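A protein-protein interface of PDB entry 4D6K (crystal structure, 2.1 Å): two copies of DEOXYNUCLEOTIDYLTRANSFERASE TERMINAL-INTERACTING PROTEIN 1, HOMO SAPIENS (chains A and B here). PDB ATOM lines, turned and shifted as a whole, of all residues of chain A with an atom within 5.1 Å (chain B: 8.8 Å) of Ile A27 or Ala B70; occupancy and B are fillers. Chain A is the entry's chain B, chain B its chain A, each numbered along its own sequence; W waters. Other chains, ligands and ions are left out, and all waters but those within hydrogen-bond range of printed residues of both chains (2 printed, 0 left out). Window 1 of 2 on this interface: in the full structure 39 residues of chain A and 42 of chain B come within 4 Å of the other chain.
The side-chain amino group (NZ) of Lys B33 is in salt-bridge range of the side-chain carboxylate (OE1) of Glu A26. NE2 of Gln A20 is in hydrogen-bond range of O of Cys B66 (3.0 Å). OE2 of Glu A26 is in hydrogen-bond range of OH of Tyr B34 (2.9 Å). O of Pro B89 sits at hydrogen-bond distance from ND2 of Asn A24, at 2.7 Å.
Hydrophobic or aromatic side chains of chain B within 4 Å of the printed part of chain A: Val B30, Tyr B34, Leu B67, Ala B70, Leu B73, Phe B74 and Pro B89. Hydrophobic or aromatic side chains of chain A that line the printed part of chain B: Ile A23, Ile A27, Val A30, Phe A31 and Leu A67. Along chain A the printed residues that touch a printed residue of chain B span positions 20 to 67. Among the printed residues, 19 pairs touch across the chains.
Water W1 bridges the backbone carbonyl oxygen of Leu B73 (2.4 Å) and the side-chain amide oxygen of Gln A28 (2.6 Å). Water W2 bridges O of Gln B69 (2.8 Å) and ND2 of Asn A24 (3.0 Å).
NE2 of Gln A28 is in hydrogen-bond range of OD1 of Asn A32. The side-chain carboxylate (OE1) of Glu B68 is in salt-bridge range of the side-chain amino group (NZ) of Lys B71, at 2.8 Å. OG of Ser B75 sits at hydrogen-bond distance from O of Lys B71. The side-chain amide oxygen (OD1) of Asn A24 lies within hydrogen-bond range of the side-chain amide nitrogen (NE2) of Gln A20 (2.9 Å).
Printed residues of chain B within 4 Å of Ile A23: Tyr B34 and Cys B66. Glu A25 touches none of the printed residues of chain B. Of chain B, only Ala B70 (3.9 Å) and Leu B73 (3.97 Å) come within 4 Å of Ile A27. Of the printed residues of chain B, Leu A67 touches Leu B67 (3.9 Å), Ala B70 (3.5 Å) and Lys B71 (3.6 Å). Of the printed residues of chain A, Cys B66 touches Gln A20 and Ile A23. Glu B68 touches none of the printed residues of chain A. Of the printed residues of chain A, Gln B69 touches Gln A20 (3.5 Å). Ala B70 touches just these residues of chain A: Gln A20 (3.6 Å), Asn A24 (3.5 Å), Ile A27 (3.9 Å) and Leu A67 (3.5 Å). Of the printed residues of chain A, Pro B89 touches Asn A24. The nearest residue of chain B that does not touch Ile A27 is Leu B67 (4.3 Å). The nearest printed residue of chain A that does not touch Phe B74 is Leu A67 (4.02 Å).
Among the printed residues, merely in contact across the chains: Gln A20 with Gln B69, Gln A20 with Ala B70, Ile A23 with Tyr B34, Ile A23 with Cys B66, Asn A24 with Ala B70, Asn A24 with Leu B73, Glu A26 with Val B30, Ile A27 with Ala B70, Ile A27 with Leu B73, Gln A28 with Leu B73, Val A30 with Glu B26, Phe A31 with Phe B74, Leu A67 with Leu B67, Leu A67 with Ala B70 and Leu A67 with Lys B71.
Glu A26 touches Val B30, and with the chains exchanged Val A30 touches Glu B26. Leu A67 touches its own counterpart, Leu B67. 7 positions are printed for both chains.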
ATOM      1  N   GLN A  20     -27.897  25.564   0.039  1.00  0.00           N
ATOM      2  CA  GLN A  20     -27.026  24.614   0.736  1.00  0.00           C
ATOM      3  C   GLN A  20     -27.481  23.156   0.763  1.00  0.00           C
ATOM      4  O   GLN A  20     -26.641  22.266   0.563  1.00  0.00           O
ATOM      5  CB  GLN A  20     -26.728  25.108   2.132  1.00  0.00           C
ATOM      6  CG  GLN A  20     -25.540  24.454   2.816  1.00  0.00           C
ATOM      7  CD  GLN A  20     -24.158  24.967   2.253  1.00  0.00           C
ATOM      8  OE1 GLN A  20     -23.938  26.158   2.104  1.00  0.00           O
ATOM      9  NE2 GLN A  20     -23.319  24.090   1.932  1.00  0.00           N
ATOM     10  N   ILE A  23     -26.821  21.651  -2.636  1.00  0.00           N
ATOM     11  CA  ILE A  23     -25.392  21.607  -2.889  1.00  0.00           C
ATOM     12  C   ILE A  23     -24.733  20.530  -2.011  1.00  0.00           C
ATOM     13  O   ILE A  23     -23.963  19.731  -2.521  1.00  0.00           O
ATOM     14  CB  ILE A  23     -24.748  22.973  -2.733  1.00  0.00           C
ATOM     15  CG1 ILE A  23     -25.239  23.917  -3.840  1.00  0.00           C
ATOM     16  CG2 ILE A  23     -23.233  22.858  -2.775  1.00  0.00           C
ATOM     17  CD1 ILE A  23     -24.818  25.378  -3.669  1.00  0.00           C
ATOM     18  N   ASN A  24     -25.079  20.467  -0.717  1.00  0.00           N
ATOM     19  CA  ASN A  24     -24.622  19.384   0.136  1.00  0.00           C
ATOM     20  C   ASN A  24     -24.890  17.964  -0.444  1.00  0.00           C
ATOM     21  O   ASN A  24     -24.034  17.114  -0.358  1.00  0.00           O
ATOM     22  CB  ASN A  24     -25.236  19.428   1.553  1.00  0.00           C
ATOM     23  CG  ASN A  24     -24.598  20.514   2.419  1.00  0.00           C
ATOM     24  OD1 ASN A  24     -23.606  21.186   2.033  1.00  0.00           O
ATOM     25  ND2 ASN A  24     -25.189  20.721   3.569  1.00  0.00           N
ATOM     26  N   GLU A  25     -26.080  17.727  -0.932  1.00  0.00           N
ATOM     27  CA  GLU A  25     -26.441  16.426  -1.463  1.00  0.00           C
ATOM     28  C   GLU A  25     -25.528  16.061  -2.626  1.00  0.00           C
ATOM     29  O   GLU A  25     -25.046  14.952  -2.702  1.00  0.00           O
ATOM     30  CB  GLU A  25     -27.806  16.479  -2.063  1.00  0.00           C
ATOM     31  CG  GLU A  25     -28.337  15.089  -2.371  1.00  0.00           C
ATOM     32  CD  GLU A  25     -28.972  14.393  -1.173  1.00  0.00           C
ATOM     33  OE1 GLU A  25     -29.012  14.952  -0.027  1.00  0.00           O
ATOM     34  OE2 GLU A  25     -29.465  13.258  -1.401  1.00  0.00           O
ATOM     35  N   GLU A  26     -25.245  17.006  -3.486  1.00  0.00           N
ATOM     36  CA  GLU A  26     -24.369  16.718  -4.622  1.00  0.00           C
ATOM     37  C   GLU A  26     -22.934  16.558  -4.197  1.00  0.00           C
ATOM     38  O   GLU A  26     -22.219  15.697  -4.711  1.00  0.00           O
ATOM     39  CB  GLU A  26     -24.498  17.818  -5.661  1.00  0.00           C
ATOM     40  CG  GLU A  26     -25.910  17.949  -6.180  1.00  0.00           C
ATOM     41  CD  GLU A  26     -25.924  18.437  -7.619  1.00  0.00           C
ATOM     42  OE1 GLU A  26     -25.214  17.840  -8.458  1.00  0.00           O
ATOM     43  OE2 GLU A  26     -26.609  19.418  -7.912  1.00  0.00           O
ATOM     44  N   ILE A  27     -22.514  17.314  -3.176  1.00  0.00           N
ATOM     45  CA  ILE A  27     -21.164  17.156  -2.648  1.00  0.00           C
ATOM     46  C   ILE A  27     -20.984  15.804  -2.002  1.00  0.00           C
ATOM     47  O   ILE A  27     -19.963  15.125  -2.196  1.00  0.00           O
ATOM     48  CB  ILE A  27     -20.793  18.330  -1.730  1.00  0.00           C
ATOM     49  CG1 ILE A  27     -20.468  19.564  -2.560  1.00  0.00           C
ATOM     50  CG2 ILE A  27     -19.570  17.975  -0.867  1.00  0.00           C
ATOM     51  CD1 ILE A  27     -20.324  20.842  -1.745  1.00  0.00           C
ATOM     52  N   GLN A  28     -21.985  15.355  -1.249  1.00  0.00           N
ATOM     53  CA  GLN A  28     -21.932  14.028  -0.655  1.00  0.00           C
ATOM     54  C   GLN A  28     -21.780  12.956  -1.740  1.00  0.00           C
ATOM     55  O   GLN A  28     -21.009  12.037  -1.596  1.00  0.00           O
ATOM     56  CB  GLN A  28     -23.221  13.750   0.178  1.00  0.00           C
ATOM     57  CG  GLN A  28     -23.221  12.447   0.940  1.00  0.00           C
ATOM     58  CD  GLN A  28     -22.216  12.389   2.112  1.00  0.00           C
ATOM     59  OE1 GLN A  28     -22.354  13.112   3.073  1.00  0.00           O
ATOM     60  NE2 GLN A  28     -21.170  11.571   1.982  1.00  0.00           N
ATOM     61  N   THR A  29     -22.557  13.067  -2.793  1.00  0.00           N
ATOM     62  CA  THR A  29     -22.478  12.125  -3.929  1.00  0.00           C
ATOM     63  C   THR A  29     -21.084  12.129  -4.569  1.00  0.00           C
ATOM     64  O   THR A  29     -20.515  11.071  -4.816  1.00  0.00           O
ATOM     65  CB  THR A  29     -23.536  12.494  -4.976  1.00  0.00           C
ATOM     66  OG1 THR A  29     -24.809  12.350  -4.364  1.00  0.00           O
ATOM     67  CG2 THR A  29     -23.416  11.621  -6.262  1.00  0.00           C
ATOM     68  N   VAL A  30     -20.476  13.306  -4.708  1.00  0.00           N
ATOM     69  CA  VAL A  30     -19.092  13.375  -5.147  1.00  0.00           C
ATOM     70  C   VAL A  30     -18.160  12.605  -4.206  1.00  0.00           C
ATOM     71  O   VAL A  30     -17.356  11.758  -4.635  1.00  0.00           O
ATOM     72  CB  VAL A  30     -18.604  14.827  -5.327  1.00  0.00           C
ATOM     73  CG1 VAL A  30     -17.097  14.916  -5.476  1.00  0.00           C
ATOM     74  CG2 VAL A  30     -19.305  15.481  -6.497  1.00  0.00           C
ATOM     75  N   PHE A  31     -18.209  12.936  -2.932  1.00  0.00           N
ATOM     76  CA  PHE A  31     -17.285  12.329  -1.968  1.00  0.00           C
ATOM     77  C   PHE A  31     -17.467  10.836  -1.794  1.00  0.00           C
ATOM     78  O   PHE A  31     -16.472  10.124  -1.518  1.00  0.00           O
ATOM     79  CB  PHE A  31     -17.318  13.032  -0.581  1.00  0.00           C
ATOM     80  CG  PHE A  31     -16.419  14.244  -0.534  1.00  0.00           C
ATOM     81  CD1 PHE A  31     -16.807  15.448  -1.106  1.00  0.00           C
ATOM     82  CD2 PHE A  31     -15.156  14.147  -0.012  1.00  0.00           C
ATOM     83  CE1 PHE A  31     -15.946  16.575  -1.088  1.00  0.00           C
ATOM     84  CE2 PHE A  31     -14.277  15.238  -0.012  1.00  0.00           C
ATOM     85  CZ  PHE A  31     -14.687  16.465  -0.541  1.00  0.00           C
ATOM     86  N   ASN A  32     -18.692  10.342  -1.952  1.00  0.00           N
ATOM     87  CA  ASN A  32     -18.938   8.893  -1.854  1.00  0.00           C
ATOM     88  C   ASN A  32     -18.086   8.136  -2.828  1.00  0.00           C
ATOM     89  O   ASN A  32     -17.681   7.047  -2.526  1.00  0.00           O
ATOM     90  CB  ASN A  32     -20.393   8.516  -2.134  1.00  0.00           C
ATOM     91  CG  ASN A  32     -21.329   8.896  -1.013  1.00  0.00           C
ATOM     92  OD1 ASN A  32     -20.935   9.144   0.111  1.00  0.00           O
ATOM     93  ND2 ASN A  32     -22.598   8.959  -1.345  1.00  0.00           N
ATOM     94  N   LEU A  67     -12.478  20.059   1.046  1.00  0.00           N
ATOM     95  CA  LEU A  67     -13.382  21.187   0.871  1.00  0.00           C
ATOM     96  C   LEU A  67     -12.684  22.538   1.077  1.00  0.00           C
ATOM     97  O   LEU A  67     -12.943  23.509   0.349  1.00  0.00           O
ATOM     98  CB  LEU A  67     -14.584  21.079   1.841  1.00  0.00           C
ATOM     99  CG  LEU A  67     -15.520  19.899   1.548  1.00  0.00           C
ATOM    100  CD1 LEU A  67     -16.568  19.767   2.667  1.00  0.00           C
ATOM    101  CD2 LEU A  67     -16.238  20.160   0.257  1.00  0.00           C
ATOM    102  N   ILE B  23     -11.436  15.707  -7.481  1.00  0.00           N
ATOM    103  CA  ILE B  23     -12.499  16.196  -6.669  1.00  0.00           C
ATOM    104  C   ILE B  23     -12.890  17.646  -7.064  1.00  0.00           C
ATOM    105  O   ILE B  23     -14.045  17.958  -7.178  1.00  0.00           O
ATOM    106  CB  ILE B  23     -12.111  16.095  -5.166  1.00  0.00           C
ATOM    107  CG1 ILE B  23     -12.044  14.635  -4.746  1.00  0.00           C
ATOM    108  CG2 ILE B  23     -13.146  16.838  -4.300  1.00  0.00           C
ATOM    109  CD1 ILE B  23     -11.491  14.393  -3.331  1.00  0.00           C
ATOM    110  N   GLU B  26     -15.160  17.731 -10.117  1.00  0.00           N
ATOM    111  CA  GLU B  26     -16.567  17.361  -9.848  1.00  0.00           C
ATOM    112  C   GLU B  26     -17.266  18.456  -9.042  1.00  0.00           C
ATOM    113  O   GLU B  26     -18.450  18.734  -9.239  1.00  0.00           O
ATOM    114  CB  GLU B  26     -16.616  16.064  -9.113  1.00  0.00           C
ATOM    115  CG  GLU B  26     -15.992  14.935  -9.902  1.00  0.00           C
ATOM    116  CD  GLU B  26     -16.623  13.610  -9.545  1.00  0.00           C
ATOM    117  OE1 GLU B  26     -17.866  13.523  -9.532  1.00  0.00           O
ATOM    118  OE2 GLU B  26     -15.896  12.660  -9.277  1.00  0.00           O
ATOM    119  N   ILE B  27     -16.523  19.110  -8.151  1.00  0.00           N
ATOM    120  CA  ILE B  27     -17.109  20.222  -7.393  1.00  0.00           C
ATOM    121  C   ILE B  27     -17.487  21.358  -8.350  1.00  0.00           C
ATOM    122  O   ILE B  27     -18.556  22.000  -8.214  1.00  0.00           O
ATOM    123  CB  ILE B  27     -16.182  20.660  -6.214  1.00  0.00           C
ATOM    124  CG1 ILE B  27     -16.302  19.638  -5.091  1.00  0.00           C
ATOM    125  CG2 ILE B  27     -16.559  22.069  -5.676  1.00  0.00           C
ATOM    126  CD1 ILE B  27     -15.295  19.801  -4.002  1.00  0.00           C
ATOM    127  N   GLN B  28     -16.607  21.656  -9.280  1.00  0.00           N
ATOM    128  CA  GLN B  28     -16.916  22.685 -10.277  1.00  0.00           C
ATOM    129  C   GLN B  28     -18.205  22.385 -11.026  1.00  0.00           C
ATOM    130  O   GLN B  28     -19.025  23.263 -11.245  1.00  0.00           O
ATOM    131  CB  GLN B  28     -15.740  22.881 -11.256  1.00  0.00           C
ATOM    132  CG  GLN B  28     -15.888  24.055 -12.222  1.00  0.00           C
ATOM    133  CD  GLN B  28     -15.855  25.423 -11.486  1.00  0.00           C
ATOM    134  OE1 GLN B  28     -14.844  25.813 -10.925  1.00  0.00           O
ATOM    135  NE2 GLN B  28     -16.981  26.141 -11.505  1.00  0.00           N
ATOM    136  N   VAL B  30     -20.717  20.560 -10.023  1.00  0.00           N
ATOM    137  CA  VAL B  30     -21.827  20.844  -9.128  1.00  0.00           C
ATOM    138  C   VAL B  30     -22.169  22.343  -9.097  1.00  0.00           C
ATOM    139  O   VAL B  30     -23.325  22.718  -9.301  1.00  0.00           O
ATOM    140  CB  VAL B  30     -21.518  20.364  -7.694  1.00  0.00           C
ATOM    141  CG1 VAL B  30     -22.538  20.917  -6.709  1.00  0.00           C
ATOM    142  CG2 VAL B  30     -21.495  18.850  -7.651  1.00  0.00           C
ATOM    143  N   PHE B  31     -21.172  23.203  -8.824  1.00  0.00           N
ATOM    144  CA  PHE B  31     -21.426  24.625  -8.685  1.00  0.00           C
ATOM    145  C   PHE B  31     -21.916  25.303  -9.990  1.00  0.00           C
ATOM    146  O   PHE B  31     -22.726  26.242  -9.926  1.00  0.00           O
ATOM    147  CB  PHE B  31     -20.224  25.398  -8.115  1.00  0.00           C
ATOM    148  CG  PHE B  31     -20.134  25.356  -6.610  1.00  0.00           C
ATOM    149  CD1 PHE B  31     -19.592  24.270  -5.954  1.00  0.00           C
ATOM    150  CD2 PHE B  31     -20.639  26.415  -5.843  1.00  0.00           C
ATOM    151  CE1 PHE B  31     -19.574  24.221  -4.548  1.00  0.00           C
ATOM    152  CE2 PHE B  31     -20.628  26.378  -4.467  1.00  0.00           C
ATOM    153  CZ  PHE B  31     -20.088  25.277  -3.820  1.00  0.00           C
ATOM    154  N   LYS B  33     -24.139  24.292 -11.957  1.00  0.00           N
ATOM    155  CA  LYS B  33     -25.597  24.240 -11.960  1.00  0.00           C
ATOM    156  C   LYS B  33     -26.296  25.314 -11.122  1.00  0.00           C
ATOM    157  O   LYS B  33     -27.435  25.634 -11.412  1.00  0.00           O
ATOM    158  CB  LYS B  33     -26.065  22.925 -11.406  1.00  0.00           C
ATOM    159  CG  LYS B  33     -25.446  21.716 -12.071  1.00  0.00           C
ATOM    160  CD  LYS B  33     -26.026  20.443 -11.450  1.00  0.00           C
ATOM    161  CE  LYS B  33     -25.222  19.234 -11.913  1.00  0.00           C
ATOM    162  NZ  LYS B  33     -25.737  18.006 -11.251  1.00  0.00           N
ATOM    163  N   TYR B  34     -25.612  25.880 -10.119  1.00  0.00           N
ATOM    164  CA  TYR B  34     -26.185  26.893  -9.235  1.00  0.00           C
ATOM    165  C   TYR B  34     -25.706  28.290  -9.501  1.00  0.00           C
ATOM    166  O   TYR B  34     -26.199  29.272  -8.898  1.00  0.00           O
ATOM    167  CB  TYR B  34     -25.883  26.505  -7.763  1.00  0.00           C
ATOM    168  CG  TYR B  34     -26.485  25.170  -7.436  1.00  0.00           C
ATOM    169  CD1 TYR B  34     -27.796  25.078  -7.020  1.00  0.00           C
ATOM    170  CD2 TYR B  34     -25.761  23.988  -7.608  1.00  0.00           C
ATOM    171  CE1 TYR B  34     -28.372  23.853  -6.778  1.00  0.00           C
ATOM    172  CE2 TYR B  34     -26.331  22.763  -7.332  1.00  0.00           C
ATOM    173  CZ  TYR B  34     -27.633  22.707  -6.922  1.00  0.00           C
ATOM    174  OH  TYR B  34     -28.236  21.502  -6.647  1.00  0.00           O
ATOM    175  N   CYS B  63     -19.775  31.248  -2.759  1.00  0.00           N
ATOM    176  CA  CYS B  63     -19.306  29.895  -3.092  1.00  0.00           C
ATOM    177  C   CYS B  63     -18.341  29.303  -2.050  1.00  0.00           C
ATOM    178  O   CYS B  63     -18.457  28.142  -1.655  1.00  0.00           O
ATOM    179  CB  CYS B  63     -18.703  29.883  -4.494  1.00  0.00           C
ATOM    180  SG  CYS B  63     -19.916  30.127  -5.826  1.00  0.00           S
ATOM    181  N   ARG B  64     -17.356  30.083  -1.614  1.00  0.00           N
ATOM    182  CA  ARG B  64     -16.482  29.640  -0.553  1.00  0.00           C
ATOM    183  C   ARG B  64     -17.284  29.323   0.711  1.00  0.00           C
ATOM    184  O   ARG B  64     -16.936  28.379   1.429  1.00  0.00           O
ATOM    185  CB  ARG B  64     -15.375  30.693  -0.215  1.00  0.00           C
ATOM    186  CG  ARG B  64     -14.420  30.914  -1.407  1.00  0.00           C
ATOM    187  CD  ARG B  64     -13.123  31.594  -0.989  1.00  0.00           C
ATOM    188  NE  ARG B  64     -13.381  32.922  -0.457  1.00  0.00           N
ATOM    189  CZ  ARG B  64     -13.497  34.051  -1.179  1.00  0.00           C
ATOM    190  NH1 ARG B  64     -13.386  34.059  -2.506  1.00  0.00           N
ATOM    191  NH2 ARG B  64     -13.744  35.186  -0.559  1.00  0.00           N
ATOM    192  N   SER B  65     -18.256  30.171   1.052  1.00  0.00           N
ATOM    193  CA  SER B  65     -19.093  29.896   2.252  1.00  0.00           C
ATOM    194  C   SER B  65     -19.812  28.594   2.087  1.00  0.00           C
ATOM    195  O   SER B  65     -19.998  27.864   3.057  1.00  0.00           O
ATOM    196  CB  SER B  65     -20.197  30.958   2.504  1.00  0.00           C
ATOM    197  OG  SER B  65     -19.568  32.081   2.949  1.00  0.00           O
ATOM    198  N   CYS B  66     -20.267  28.287   0.857  1.00  0.00           N
ATOM    199  CA  CYS B  66     -20.957  27.017   0.629  1.00  0.00           C
ATOM    200  C   CYS B  66     -20.039  25.846   0.954  1.00  0.00           C
ATOM    201  O   CYS B  66     -20.474  24.867   1.539  1.00  0.00           O
ATOM    202  CB  CYS B  66     -21.418  26.853  -0.826  1.00  0.00           C
ATOM    203  SG  CYS B  66     -22.910  27.655  -1.344  1.00  0.00           S
ATOM    204  N   LEU B  67     -18.783  25.938   0.527  1.00  0.00           N
ATOM    205  CA  LEU B  67     -17.842  24.888   0.813  1.00  0.00           C
ATOM    206  C   LEU B  67     -17.536  24.794   2.303  1.00  0.00           C
ATOM    207  O   LEU B  67     -17.413  23.696   2.852  1.00  0.00           O
ATOM    208  CB  LEU B  67     -16.526  25.116  -0.002  1.00  0.00           C
ATOM    209  CG  LEU B  67     -16.649  24.949  -1.482  1.00  0.00           C
ATOM    210  CD1 LEU B  67     -15.356  25.399  -2.194  1.00  0.00           C
ATOM    211  CD2 LEU B  67     -16.919  23.514  -1.815  1.00  0.00           C
ATOM    212  N   GLU B  68     -17.428  25.936   2.964  1.00  0.00           N
ATOM    213  CA  GLU B  68     -17.254  25.942   4.420  1.00  0.00           C
ATOM    214  C   GLU B  68     -18.395  25.212   5.119  1.00  0.00           C
ATOM    215  O   GLU B  68     -18.164  24.321   5.973  1.00  0.00           O
ATOM    216  CB  GLU B  68     -17.137  27.401   4.952  1.00  0.00           C
ATOM    217  CG  GLU B  68     -16.931  27.534   6.472  1.00  0.00           C
ATOM    218  CD  GLU B  68     -15.655  26.867   6.969  1.00  0.00           C
ATOM    219  OE1 GLU B  68     -14.690  26.636   6.192  1.00  0.00           O
ATOM    220  OE2 GLU B  68     -15.631  26.479   8.143  1.00  0.00           O
ATOM    221  N   GLN B  69     -19.619  25.553   4.759  1.00  0.00           N
ATOM    222  CA  GLN B  69     -20.765  24.914   5.403  1.00  0.00           C
ATOM    223  C   GLN B  69     -20.873  23.431   5.064  1.00  0.00           C
ATOM    224  O   GLN B  69     -21.349  22.597   5.893  1.00  0.00           O
ATOM    225  CB  GLN B  69     -22.079  25.616   5.004  1.00  0.00           C
ATOM    226  CG  GLN B  69     -22.110  27.029   5.530  1.00  0.00           C
ATOM    227  CD  GLN B  69     -22.074  26.987   7.052  1.00  0.00           C
ATOM    228  OE1 GLN B  69     -22.826  26.256   7.704  1.00  0.00           O
ATOM    229  NE2 GLN B  69     -21.127  27.690   7.598  1.00  0.00           N
ATOM    230  N   ALA B  70     -20.441  23.070   3.856  1.00  0.00           N
ATOM    231  CA  ALA B  70     -20.423  21.643   3.484  1.00  0.00           C
ATOM    232  C   ALA B  70     -19.494  20.787   4.355  1.00  0.00           C
ATOM    233  O   ALA B  70     -19.653  19.572   4.413  1.00  0.00           O
ATOM    234  CB  ALA B  70     -20.097  21.490   2.056  1.00  0.00           C
ATOM    235  N   LYS B  71     -18.575  21.408   5.098  1.00  0.00           N
ATOM    236  CA  LYS B  71     -17.758  20.646   6.046  1.00  0.00           C
ATOM    237  C   LYS B  71     -18.582  19.976   7.137  1.00  0.00           C
ATOM    238  O   LYS B  71     -18.129  18.956   7.702  1.00  0.00           O
ATOM    239  CB  LYS B  71     -16.661  21.484   6.698  1.00  0.00           C
ATOM    240  CG  LYS B  71     -15.650  22.042   5.688  1.00  0.00           C
ATOM    241  CD  LYS B  71     -14.645  22.943   6.406  1.00  0.00           C
ATOM    242  CE  LYS B  71     -13.610  23.530   5.444  1.00  0.00           C
ATOM    243  NZ  LYS B  71     -12.783  24.566   6.141  1.00  0.00           N
ATOM    244  N   LEU B  72     -19.798  20.486   7.401  1.00  0.00           N
ATOM    245  CA  LEU B  72     -20.698  19.805   8.372  1.00  0.00           C
ATOM    246  C   LEU B  72     -21.102  18.419   7.922  1.00  0.00           C
ATOM    247  O   LEU B  72     -21.487  17.597   8.752  1.00  0.00           O
ATOM    248  CB  LEU B  72     -21.945  20.620   8.646  1.00  0.00           C
ATOM    249  CG  LEU B  72     -21.713  21.978   9.232  1.00  0.00           C
ATOM    250  CD1 LEU B  72     -23.056  22.723   9.312  1.00  0.00           C
ATOM    251  CD2 LEU B  72     -21.053  21.855  10.631  1.00  0.00           C
ATOM    252  N   LEU B  73     -20.975  18.087   6.632  1.00  0.00           N
ATOM    253  CA  LEU B  73     -21.198  16.717   6.209  1.00  0.00           C
ATOM    254  C   LEU B  73     -20.220  15.749   6.859  1.00  0.00           C
ATOM    255  O   LEU B  73     -20.502  14.565   6.921  1.00  0.00           O
ATOM    256  CB  LEU B  73     -21.050  16.541   4.708  1.00  0.00           C
ATOM    257  CG  LEU B  73     -22.098  17.245   3.867  1.00  0.00           C
ATOM    258  CD1 LEU B  73     -21.656  17.287   2.436  1.00  0.00           C
ATOM    259  CD2 LEU B  73     -23.452  16.514   4.006  1.00  0.00           C
ATOM    260  N   PHE B  74     -19.068  16.229   7.289  1.00  0.00           N
ATOM    261  CA  PHE B  74     -17.969  15.376   7.746  1.00  0.00           C
ATOM    262  C   PHE B  74     -17.504  15.842   9.125  1.00  0.00           C
ATOM    263  O   PHE B  74     -16.309  16.000   9.364  1.00  0.00           O
ATOM    264  CB  PHE B  74     -16.788  15.508   6.777  1.00  0.00           C
ATOM    265  CG  PHE B  74     -17.150  15.199   5.378  1.00  0.00           C
ATOM    266  CD1 PHE B  74     -17.500  13.908   5.027  1.00  0.00           C
ATOM    267  CD2 PHE B  74     -17.165  16.178   4.420  1.00  0.00           C
ATOM    268  CE1 PHE B  74     -17.852  13.604   3.725  1.00  0.00           C
ATOM    269  CE2 PHE B  74     -17.534  15.887   3.126  1.00  0.00           C
ATOM    270  CZ  PHE B  74     -17.911  14.604   2.778  1.00  0.00           C
ATOM    271  N   SER B  75     -18.455  16.144   9.990  1.00  0.00           N
ATOM    272  CA  SER B  75     -18.168  16.590  11.365  1.00  0.00           C
ATOM    273  C   SER B  75     -18.998  15.654  12.279  1.00  0.00           C
ATOM    274  O   SER B  75     -19.870  14.926  11.807  1.00  0.00           O
ATOM    275  CB  SER B  75     -18.463  18.090  11.519  1.00  0.00           C
ATOM    276  OG  SER B  75     -17.696  18.898  10.567  1.00  0.00           O
ATOM    277  N   LEU B  88     -28.106  17.547   9.186  1.00  0.00           N
ATOM    278  CA  LEU B  88     -27.399  18.293   8.126  1.00  0.00           C
ATOM    279  C   LEU B  88     -28.328  18.813   7.057  1.00  0.00           C
ATOM    280  O   LEU B  88     -29.110  18.035   6.542  1.00  0.00           O
ATOM    281  CB  LEU B  88     -26.427  17.370   7.400  1.00  0.00           C
ATOM    282  CG  LEU B  88     -25.033  17.644   7.836  1.00  0.00           C
ATOM    283  CD1 LEU B  88     -24.645  18.996   7.251  1.00  0.00           C
ATOM    284  CD2 LEU B  88     -24.902  17.539   9.368  1.00  0.00           C
ATOM    285  N   PRO B  89     -28.208  20.103   6.665  1.00  0.00           N
ATOM    286  CA  PRO B  89     -29.025  20.527   5.476  1.00  0.00           C
ATOM    287  C   PRO B  89     -28.710  19.565   4.276  1.00  0.00           C
ATOM    288  O   PRO B  89     -27.517  19.368   3.907  1.00  0.00           O
ATOM    289  CB  PRO B  89     -28.561  21.971   5.239  1.00  0.00           C
ATOM    290  CG  PRO B  89     -28.040  22.449   6.580  1.00  0.00           C
ATOM    291  CD  PRO B  89     -27.405  21.227   7.220  1.00  0.00           C
HETATM  292  O   HOH W   1     -21.949  13.090   5.641  1.00  0.00           O
HETATM  293  O   HOH W   2     -24.192  22.483   5.838  1.00  0.00           O
